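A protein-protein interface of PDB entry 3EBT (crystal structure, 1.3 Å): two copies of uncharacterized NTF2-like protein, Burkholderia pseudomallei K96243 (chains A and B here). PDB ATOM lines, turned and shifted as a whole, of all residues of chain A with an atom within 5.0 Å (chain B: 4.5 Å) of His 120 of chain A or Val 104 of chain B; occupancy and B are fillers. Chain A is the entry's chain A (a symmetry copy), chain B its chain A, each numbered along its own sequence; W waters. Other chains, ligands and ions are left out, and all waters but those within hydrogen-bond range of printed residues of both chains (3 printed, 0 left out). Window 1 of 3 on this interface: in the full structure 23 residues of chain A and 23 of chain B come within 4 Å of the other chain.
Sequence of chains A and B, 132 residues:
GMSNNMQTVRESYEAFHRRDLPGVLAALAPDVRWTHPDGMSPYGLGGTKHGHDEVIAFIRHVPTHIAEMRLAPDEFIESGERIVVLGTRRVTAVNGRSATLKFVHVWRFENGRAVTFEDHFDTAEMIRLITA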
ATOM      1  N   PRO A  37     -29.667 -36.264  -5.223  1.00  0.00           N
ATOM      2  CA  PRO A  37     -29.997 -35.417  -4.081  1.00  0.00           C
ATOM      3  C   PRO A  37     -30.307 -36.193  -2.810  1.00  0.00           C
ATOM      4  O   PRO A  37     -30.986 -37.218  -2.850  1.00  0.00           O
ATOM      5  CB  PRO A  37     -31.224 -34.648  -4.573  1.00  0.00           C
ATOM      6  CG  PRO A  37     -31.092 -34.632  -6.053  1.00  0.00           C
ATOM      7  CD  PRO A  37     -30.546 -35.990  -6.373  1.00  0.00           C
ATOM      8  N   LYS A 102     -37.528 -31.455 -14.956  1.00  0.00           N
ATOM      9  CA  LYS A 102     -36.265 -30.863 -15.391  1.00  0.00           C
ATOM     10  C   LYS A 102     -35.096 -31.580 -14.742  1.00  0.00           C
ATOM     11  O   LYS A 102     -35.228 -32.128 -13.645  1.00  0.00           O
ATOM     12  CB  LYS A 102     -36.223 -29.368 -15.023  1.00  0.00           C
ATOM     13  CG  LYS A 102     -37.206 -28.531 -15.815  1.00  0.00           C
ATOM     14  CD  LYS A 102     -37.143 -27.086 -15.508  1.00  0.00           C
ATOM     15  CE  LYS A 102     -37.775 -26.675 -14.252  1.00  0.00           C
ATOM     16  NZ  LYS A 102     -37.987 -25.142 -14.238  1.00  0.00           N
ATOM     17  N   PHE A 103     -33.961 -31.561 -15.413  1.00  0.00           N
ATOM     18  CA  PHE A 103     -32.730 -32.031 -14.806  1.00  0.00           C
ATOM     19  C   PHE A 103     -31.552 -31.148 -15.149  1.00  0.00           C
ATOM     20  O   PHE A 103     -31.555 -30.470 -16.178  1.00  0.00           O
ATOM     21  CB  PHE A 103     -32.429 -33.499 -15.196  1.00  0.00           C
ATOM     22  CG  PHE A 103     -31.933 -33.695 -16.609  1.00  0.00           C
ATOM     23  CD1 PHE A 103     -30.574 -33.581 -16.892  1.00  0.00           C
ATOM     24  CD2 PHE A 103     -32.794 -33.958 -17.661  1.00  0.00           C
ATOM     25  CE1 PHE A 103     -30.116 -33.731 -18.192  1.00  0.00           C
ATOM     26  CE2 PHE A 103     -32.324 -34.115 -18.958  1.00  0.00           C
ATOM     27  CZ  PHE A 103     -30.985 -34.004 -19.207  1.00  0.00           C
ATOM     28  N   VAL A 104     -30.544 -31.181 -14.281  1.00  0.00           N
ATOM     29  CA  VAL A 104     -29.236 -30.622 -14.543  1.00  0.00           C
ATOM     30  C   VAL A 104     -28.221 -31.700 -14.130  1.00  0.00           C
ATOM     31  O   VAL A 104     -28.258 -32.182 -13.006  1.00  0.00           O
ATOM     32  CB  VAL A 104     -28.966 -29.351 -13.751  1.00  0.00           C
ATOM     33  CG1 VAL A 104     -27.530 -28.868 -13.987  1.00  0.00           C
ATOM     34  CG2 VAL A 104     -29.981 -28.251 -14.151  1.00  0.00           C
ATOM     35  N   VAL A 106     -24.136 -32.503 -13.867  1.00  0.00           N
ATOM     36  CA  VAL A 106     -22.796 -31.948 -13.779  1.00  0.00           C
ATOM     37  C   VAL A 106     -21.800 -33.119 -13.932  1.00  0.00           C
ATOM     38  O   VAL A 106     -21.859 -34.038 -13.134  1.00  0.00           O
ATOM     39  CB  VAL A 106     -22.614 -31.223 -12.406  1.00  0.00           C
ATOM     40  CG1 VAL A 106     -21.194 -30.652 -12.242  1.00  0.00           C
ATOM     41  CG2 VAL A 106     -23.640 -30.050 -12.263  1.00  0.00           C
ATOM     42  N   GLU A 118     -23.221 -35.613 -11.064  1.00  0.00           N
ATOM     43  CA  GLU A 118     -24.265 -35.277 -10.122  1.00  0.00           C
ATOM     44  C   GLU A 118     -25.507 -34.781 -10.857  1.00  0.00           C
ATOM     45  O   GLU A 118     -25.407 -33.985 -11.794  1.00  0.00           O
ATOM     46  CB  GLU A 118     -23.789 -34.224  -9.117  1.00  0.00           C
ATOM     47  CG  GLU A 118     -24.803 -33.953  -8.036  1.00  0.00           C
ATOM     48  CD  GLU A 118     -24.272 -33.261  -6.785  1.00  0.00           C
ATOM     49  OE1 GLU A 118     -23.045 -33.078  -6.681  1.00  0.00           O
ATOM     50  OE2 GLU A 118     -25.099 -32.934  -5.914  1.00  0.00           O
ATOM     51  N   ASP A 119     -26.655 -35.260 -10.385  1.00  0.00           N
ATOM     52  CA  ASP A 119     -27.969 -34.889 -10.918  1.00  0.00           C
ATOM     53  C   ASP A 119     -28.641 -33.978  -9.882  1.00  0.00           C
ATOM     54  O   ASP A 119     -28.779 -34.348  -8.718  1.00  0.00           O
ATOM     55  CB  ASP A 119     -28.774 -36.185 -11.152  1.00  0.00           C
ATOM     56  CG  ASP A 119     -30.012 -36.010 -11.985  1.00  0.00           C
ATOM     57  OD1 ASP A 119     -30.520 -34.907 -12.163  1.00  0.00           O
ATOM     58  OD2 ASP A 119     -30.484 -37.070 -12.462  1.00  0.00           O
ATOM     59  N   HIS A 120     -28.996 -32.770 -10.322  1.00  0.00           N
ATOM     60  CA  HIS A 120     -29.667 -31.758  -9.512  1.00  0.00           C
ATOM     61  C   HIS A 120     -31.070 -31.543 -10.076  1.00  0.00           C
ATOM     62  O   HIS A 120     -31.230 -31.279 -11.284  1.00  0.00           O
ATOM     63  CB  HIS A 120     -28.912 -30.433  -9.584  1.00  0.00           C
ATOM     64  CG  HIS A 120     -27.521 -30.445  -9.046  1.00  0.00           C
ATOM     65  ND1 HIS A 120     -27.221 -29.976  -7.778  1.00  0.00           N
ATOM     66  CD2 HIS A 120     -26.350 -30.789  -9.631  1.00  0.00           C
ATOM     67  CE1 HIS A 120     -25.909 -30.073  -7.620  1.00  0.00           C
ATOM     68  NE2 HIS A 120     -25.356 -30.546  -8.721  1.00  0.00           N
ATOM     69  N   PHE A 121     -32.063 -31.611  -9.209  1.00  0.00           N
ATOM     70  CA  PHE A 121     -33.456 -31.454  -9.629  1.00  0.00           C
ATOM     71  C   PHE A 121     -34.393 -31.219  -8.448  1.00  0.00           C
ATOM     72  O   PHE A 121     -34.038 -31.373  -7.279  1.00  0.00           O
ATOM     73  CB  PHE A 121     -33.909 -32.683 -10.438  1.00  0.00           C
ATOM     74  CG  PHE A 121     -33.819 -33.977  -9.685  1.00  0.00           C
ATOM     75  CD1 PHE A 121     -32.659 -34.742  -9.705  1.00  0.00           C
ATOM     76  CD2 PHE A 121     -34.885 -34.458  -8.948  1.00  0.00           C
ATOM     77  CE1 PHE A 121     -32.577 -35.945  -9.073  1.00  0.00           C
ATOM     78  CE2 PHE A 121     -34.805 -35.662  -8.271  1.00  0.00           C
ATOM     79  CZ  PHE A 121     -33.680 -36.422  -8.364  1.00  0.00           C
ATOM     80  N   ASP A 122     -35.620 -30.869  -8.809  1.00  0.00           N
ATOM     81  CA  ASP A 122     -36.718 -30.578  -7.884  1.00  0.00           C
ATOM     82  C   ASP A 122     -37.202 -31.897  -7.307  1.00  0.00           C
ATOM     83  O   ASP A 122     -38.034 -32.604  -7.867  1.00  0.00           O
ATOM     84  CB  ASP A 122     -37.810 -29.835  -8.669  1.00  0.00           C
ATOM     85  CG  ASP A 122     -38.944 -29.284  -7.823  1.00  0.00           C
ATOM     86  OD1 ASP A 122     -39.219 -29.823  -6.726  1.00  0.00           O
ATOM     87  OD2 ASP A 122     -39.593 -28.333  -8.330  1.00  0.00           O
ATOM     88  N   VAL B  84     -22.816 -21.375 -15.823  1.00  0.00           N
ATOM     89  CA  VAL B  84     -23.389 -22.199 -14.754  1.00  0.00           C
ATOM     90  C   VAL B  84     -22.504 -22.016 -13.541  1.00  0.00           C
ATOM     91  O   VAL B  84     -21.268 -22.111 -13.625  1.00  0.00           O
ATOM     92  CB  VAL B  84     -23.485 -23.665 -15.130  1.00  0.00           C
ATOM     93  CG1 VAL B  84     -24.076 -24.489 -13.971  1.00  0.00           C
ATOM     94  CG2 VAL B  84     -24.328 -23.851 -16.380  1.00  0.00           C
ATOM     95  N   VAL B  85     -23.125 -21.717 -12.406  1.00  0.00           N
ATOM     96  CA  VAL B  85     -22.429 -21.544 -11.135  1.00  0.00           C
ATOM     97  C   VAL B  85     -22.909 -22.658 -10.193  1.00  0.00           C
ATOM     98  O   VAL B  85     -24.112 -22.893 -10.030  1.00  0.00           O
ATOM     99  CB  VAL B  85     -22.719 -20.194 -10.513  1.00  0.00           C
ATOM    100  CG1 VAL B  85     -21.902 -19.984  -9.231  1.00  0.00           C
ATOM    101  CG2 VAL B  85     -22.418 -19.048 -11.534  1.00  0.00           C
ATOM    102  N   LEU B  86     -21.955 -23.347  -9.590  1.00  0.00           N
ATOM    103  CA  LEU B  86     -22.327 -24.326  -8.573  1.00  0.00           C
ATOM    104  C   LEU B  86     -21.687 -23.953  -7.277  1.00  0.00           C
ATOM    105  O   LEU B  86     -20.619 -23.344  -7.213  1.00  0.00           O
ATOM    106  CB  LEU B  86     -21.989 -25.749  -8.950  1.00  0.00           C
ATOM    107  CG  LEU B  86     -22.572 -26.221 -10.278  1.00  0.00           C
ATOM    108  CD1 LEU B  86     -21.609 -25.892 -11.415  1.00  0.00           C
ATOM    109  CD2 LEU B  86     -22.809 -27.706 -10.210  1.00  0.00           C
ATOM    110  N   PHE B 103     -26.580 -25.418  -4.408  1.00  0.00           N
ATOM    111  CA  PHE B 103     -27.287 -24.744  -5.482  1.00  0.00           C
ATOM    112  C   PHE B 103     -26.582 -24.894  -6.811  1.00  0.00           C
ATOM    113  O   PHE B 103     -25.368 -25.101  -6.857  1.00  0.00           O
ATOM    114  CB  PHE B 103     -27.510 -23.245  -5.161  1.00  0.00           C
ATOM    115  CG  PHE B 103     -26.279 -22.378  -5.281  1.00  0.00           C
ATOM    116  CD1 PHE B 103     -25.933 -21.828  -6.513  1.00  0.00           C
ATOM    117  CD2 PHE B 103     -25.449 -22.126  -4.202  1.00  0.00           C
ATOM    118  CE1 PHE B 103     -24.789 -21.053  -6.635  1.00  0.00           C
ATOM    119  CE2 PHE B 103     -24.309 -21.343  -4.334  1.00  0.00           C
ATOM    120  CZ  PHE B 103     -23.996 -20.810  -5.553  1.00  0.00           C
ATOM    121  N   VAL B 104     -27.359 -24.771  -7.884  1.00  0.00           N
ATOM    122  CA  VAL B 104     -26.855 -24.625  -9.232  1.00  0.00           C
ATOM    123  C   VAL B 104     -27.634 -23.455  -9.854  1.00  0.00           C
ATOM    124  O   VAL B 104     -28.857 -23.464  -9.858  1.00  0.00           O
ATOM    125  CB  VAL B 104     -27.061 -25.871 -10.079  1.00  0.00           C
ATOM    126  CG1 VAL B 104     -26.607 -25.618 -11.523  1.00  0.00           C
ATOM    127  CG2 VAL B 104     -26.285 -27.064  -9.468  1.00  0.00           C
ATOM    128  N   HIS B 105     -26.902 -22.449 -10.314  1.00  0.00           N
ATOM    129  CA  HIS B 105     -27.500 -21.321 -11.023  1.00  0.00           C
ATOM    130  C   HIS B 105     -27.094 -21.363 -12.479  1.00  0.00           C
ATOM    131  O   HIS B 105     -25.896 -21.478 -12.796  1.00  0.00           O
ATOM    132  CB  HIS B 105     -26.998 -20.009 -10.450  1.00  0.00           C
ATOM    133  CG  HIS B 105     -27.492 -19.731  -9.070  1.00  0.00           C
ATOM    134  ND1 HIS B 105     -26.994 -18.704  -8.302  1.00  0.00           N
ATOM    135  CD2 HIS B 105     -28.475 -20.298  -8.341  1.00  0.00           C
ATOM    136  CE1 HIS B 105     -27.645 -18.668  -7.161  1.00  0.00           C
ATOM    137  NE2 HIS B 105     -28.541 -19.634  -7.147  1.00  0.00           N
ATOM    138  N   VAL B 106     -28.070 -21.231 -13.356  1.00  0.00           N
ATOM    139  CA  VAL B 106     -27.887 -21.193 -14.798  1.00  0.00           C
ATOM    140  C   VAL B 106     -28.186 -19.751 -15.263  1.00  0.00           C
ATOM    141  O   VAL B 106     -29.288 -19.284 -15.031  1.00  0.00           O
ATOM    142  CB  VAL B 106     -28.848 -22.221 -15.480  1.00  0.00           C
ATOM    143  CG1 VAL B 106     -28.725 -22.192 -17.013  1.00  0.00           C
ATOM    144  CG2 VAL B 106     -28.539 -23.673 -14.984  1.00  0.00           C
ATOM    145  N   GLU B 118     -31.857 -19.240 -13.610  1.00  0.00           N
ATOM    146  CA  GLU B 118     -32.617 -20.278 -12.950  1.00  0.00           C
ATOM    147  C   GLU B 118     -31.783 -20.932 -11.853  1.00  0.00           C
ATOM    148  O   GLU B 118     -30.603 -21.231 -12.052  1.00  0.00           O
ATOM    149  CB  GLU B 118     -33.099 -21.333 -13.949  1.00  0.00           C
ATOM    150  CG  GLU B 118     -34.011 -22.354 -13.320  1.00  0.00           C
ATOM    151  CD  GLU B 118     -34.862 -23.170 -14.286  1.00  0.00           C
ATOM    152  OE1 GLU B 118     -34.846 -22.869 -15.494  1.00  0.00           O
ATOM    153  OE2 GLU B 118     -35.553 -24.088 -13.809  1.00  0.00           O
ATOM    154  N   ASP B 119     -32.442 -21.157 -10.719  1.00  0.00           N
ATOM    155  CA  ASP B 119     -31.846 -21.807  -9.549  1.00  0.00           C
ATOM    156  C   ASP B 119     -32.450 -23.215  -9.452  1.00  0.00           C
ATOM    157  O   ASP B 119     -33.668 -23.373  -9.412  1.00  0.00           O
ATOM    158  CB  ASP B 119     -32.177 -20.954  -8.306  1.00  0.00           C
ATOM    159  CG  ASP B 119     -31.382 -21.301  -7.080  1.00  0.00           C
ATOM    160  OD1 ASP B 119     -30.793 -22.373  -6.974  1.00  0.00           O
ATOM    161  OD2 ASP B 119     -31.386 -20.426  -6.181  1.00  0.00           O
ATOM    162  N   HIS B 120     -31.573 -24.220  -9.475  1.00  0.00           N
ATOM    163  CA  HIS B 120     -31.929 -25.632  -9.373  1.00  0.00           C
ATOM    164  C   HIS B 120     -31.369 -26.176  -8.060  1.00  0.00           C
ATOM    165  O   HIS B 120     -30.162 -26.032  -7.781  1.00  0.00           O
ATOM    166  CB  HIS B 120     -31.308 -26.421 -10.523  1.00  0.00           C
ATOM    167  CG  HIS B 120     -31.763 -26.045 -11.893  1.00  0.00           C
ATOM    168  ND1 HIS B 120     -32.726 -26.772 -12.572  1.00  0.00           N
ATOM    169  CD2 HIS B 120     -31.329 -25.076 -12.733  1.00  0.00           C
ATOM    170  CE1 HIS B 120     -32.869 -26.220 -13.768  1.00  0.00           C
ATOM    171  NE2 HIS B 120     -32.034 -25.206 -13.900  1.00  0.00           N
HETATM  172  O   HOH W   1     -33.238 -29.581 -12.584  1.00  0.00           O
HETATM  173  O   HOH W   2     -37.192 -23.584 -16.768  1.00  0.00           O
HETATM  174  O   HOH W   3     -28.353 -27.808  -6.306  1.00  0.00           O
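The side-chain carboxylate (OE2) of Glu 118 of chain B lies within salt-bridge range of the side-chain amino group (NZ) of Lys 102 of chain A (2.7 Å).
Water W2 bridges OE1 of Glu 118 of chain B (2.8 Å) and NZ of Lys 102 of chain A (3.1 Å). Water W3 bridges ND1 of His 120 of chain A (2.9 Å) and O of His 120 of chain B (2.9 Å). Water W1 lies within hydrogen-bond range of a ring nitrogen (ND1) of His 120 of chain B (2.9 Å), the backbone carbonyl oxygen (O) of His 120 of chain A (2.9 Å) and the backbone carbonyl oxygen (O) of Lys 102 of chain A (3.4 Å).
Val 104 of chain A touches His 120 of chain B, and with the chains exchanged His 120 of chain A touches Val 104 of chain B.
Val 104 of chain A touches His 120 of chain B. Val 106 of chain A touches Leu 86 of chain B. ND1 of His 120 of chain A touches CG2 of Val 104 of chain B, 3.5 Å away.
Printed residues of chain B that touch a printed residue of chain A: Leu 86, Val 104, Glu 118 and His 120. Of the 10 printed residues of chain A, 4 touch a printed residue of chain B. Along chain A the printed residues that touch a printed residue of chain B span positions 102 to 120. Among the printed residues, 4 pairs touch across the chains. Among the printed residues, Asp or Glu carboxylates within 4 Å of a Lys or Arg side-chain nitrogen of the other chain: Lys 102 of chain A with Glu 118 of chain B (2.7 Å).
Of the printed residues of chain B, Lys 102 of chain A touches Glu 118 (2.7 Å). Of the printed residues of chain B, Val 106 of chain A touches Leu 86. Printed residues of chain A within 4 Å of Leu 86 of chain B: Val 106 (3.2 Å). Printed residues of chain B within 4 Å of Val 104 of chain A: His 120 (3.5 Å). Asp 119 of chain B touches none of the printed residues of chain A. The nearest residue of chain A that does not touch Val 104 of chain B is Val 104 of chain A (4.2 Å).
The backbone NH (N) of His 120 of chain A sits at hydrogen-bond distance from the backbone carbonyl oxygen (O) of Val 104 of chain A, 2.8 Å away. The backbone carbonyl oxygen (O) of Val 104 of chain B lies within hydrogen-bond range of the backbone NH (N) of His 120 of chain B, at 2.8 Å. The backbone carbonyl oxygen (O) of Glu 118 of chain B lies within hydrogen-bond range of the backbone NH (N) of Val 106 of chain B, at 2.8 Å. O of Glu 118 of chain A sits at hydrogen-bond distance from N of Val 106 of chain A, 2.8 Å away.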
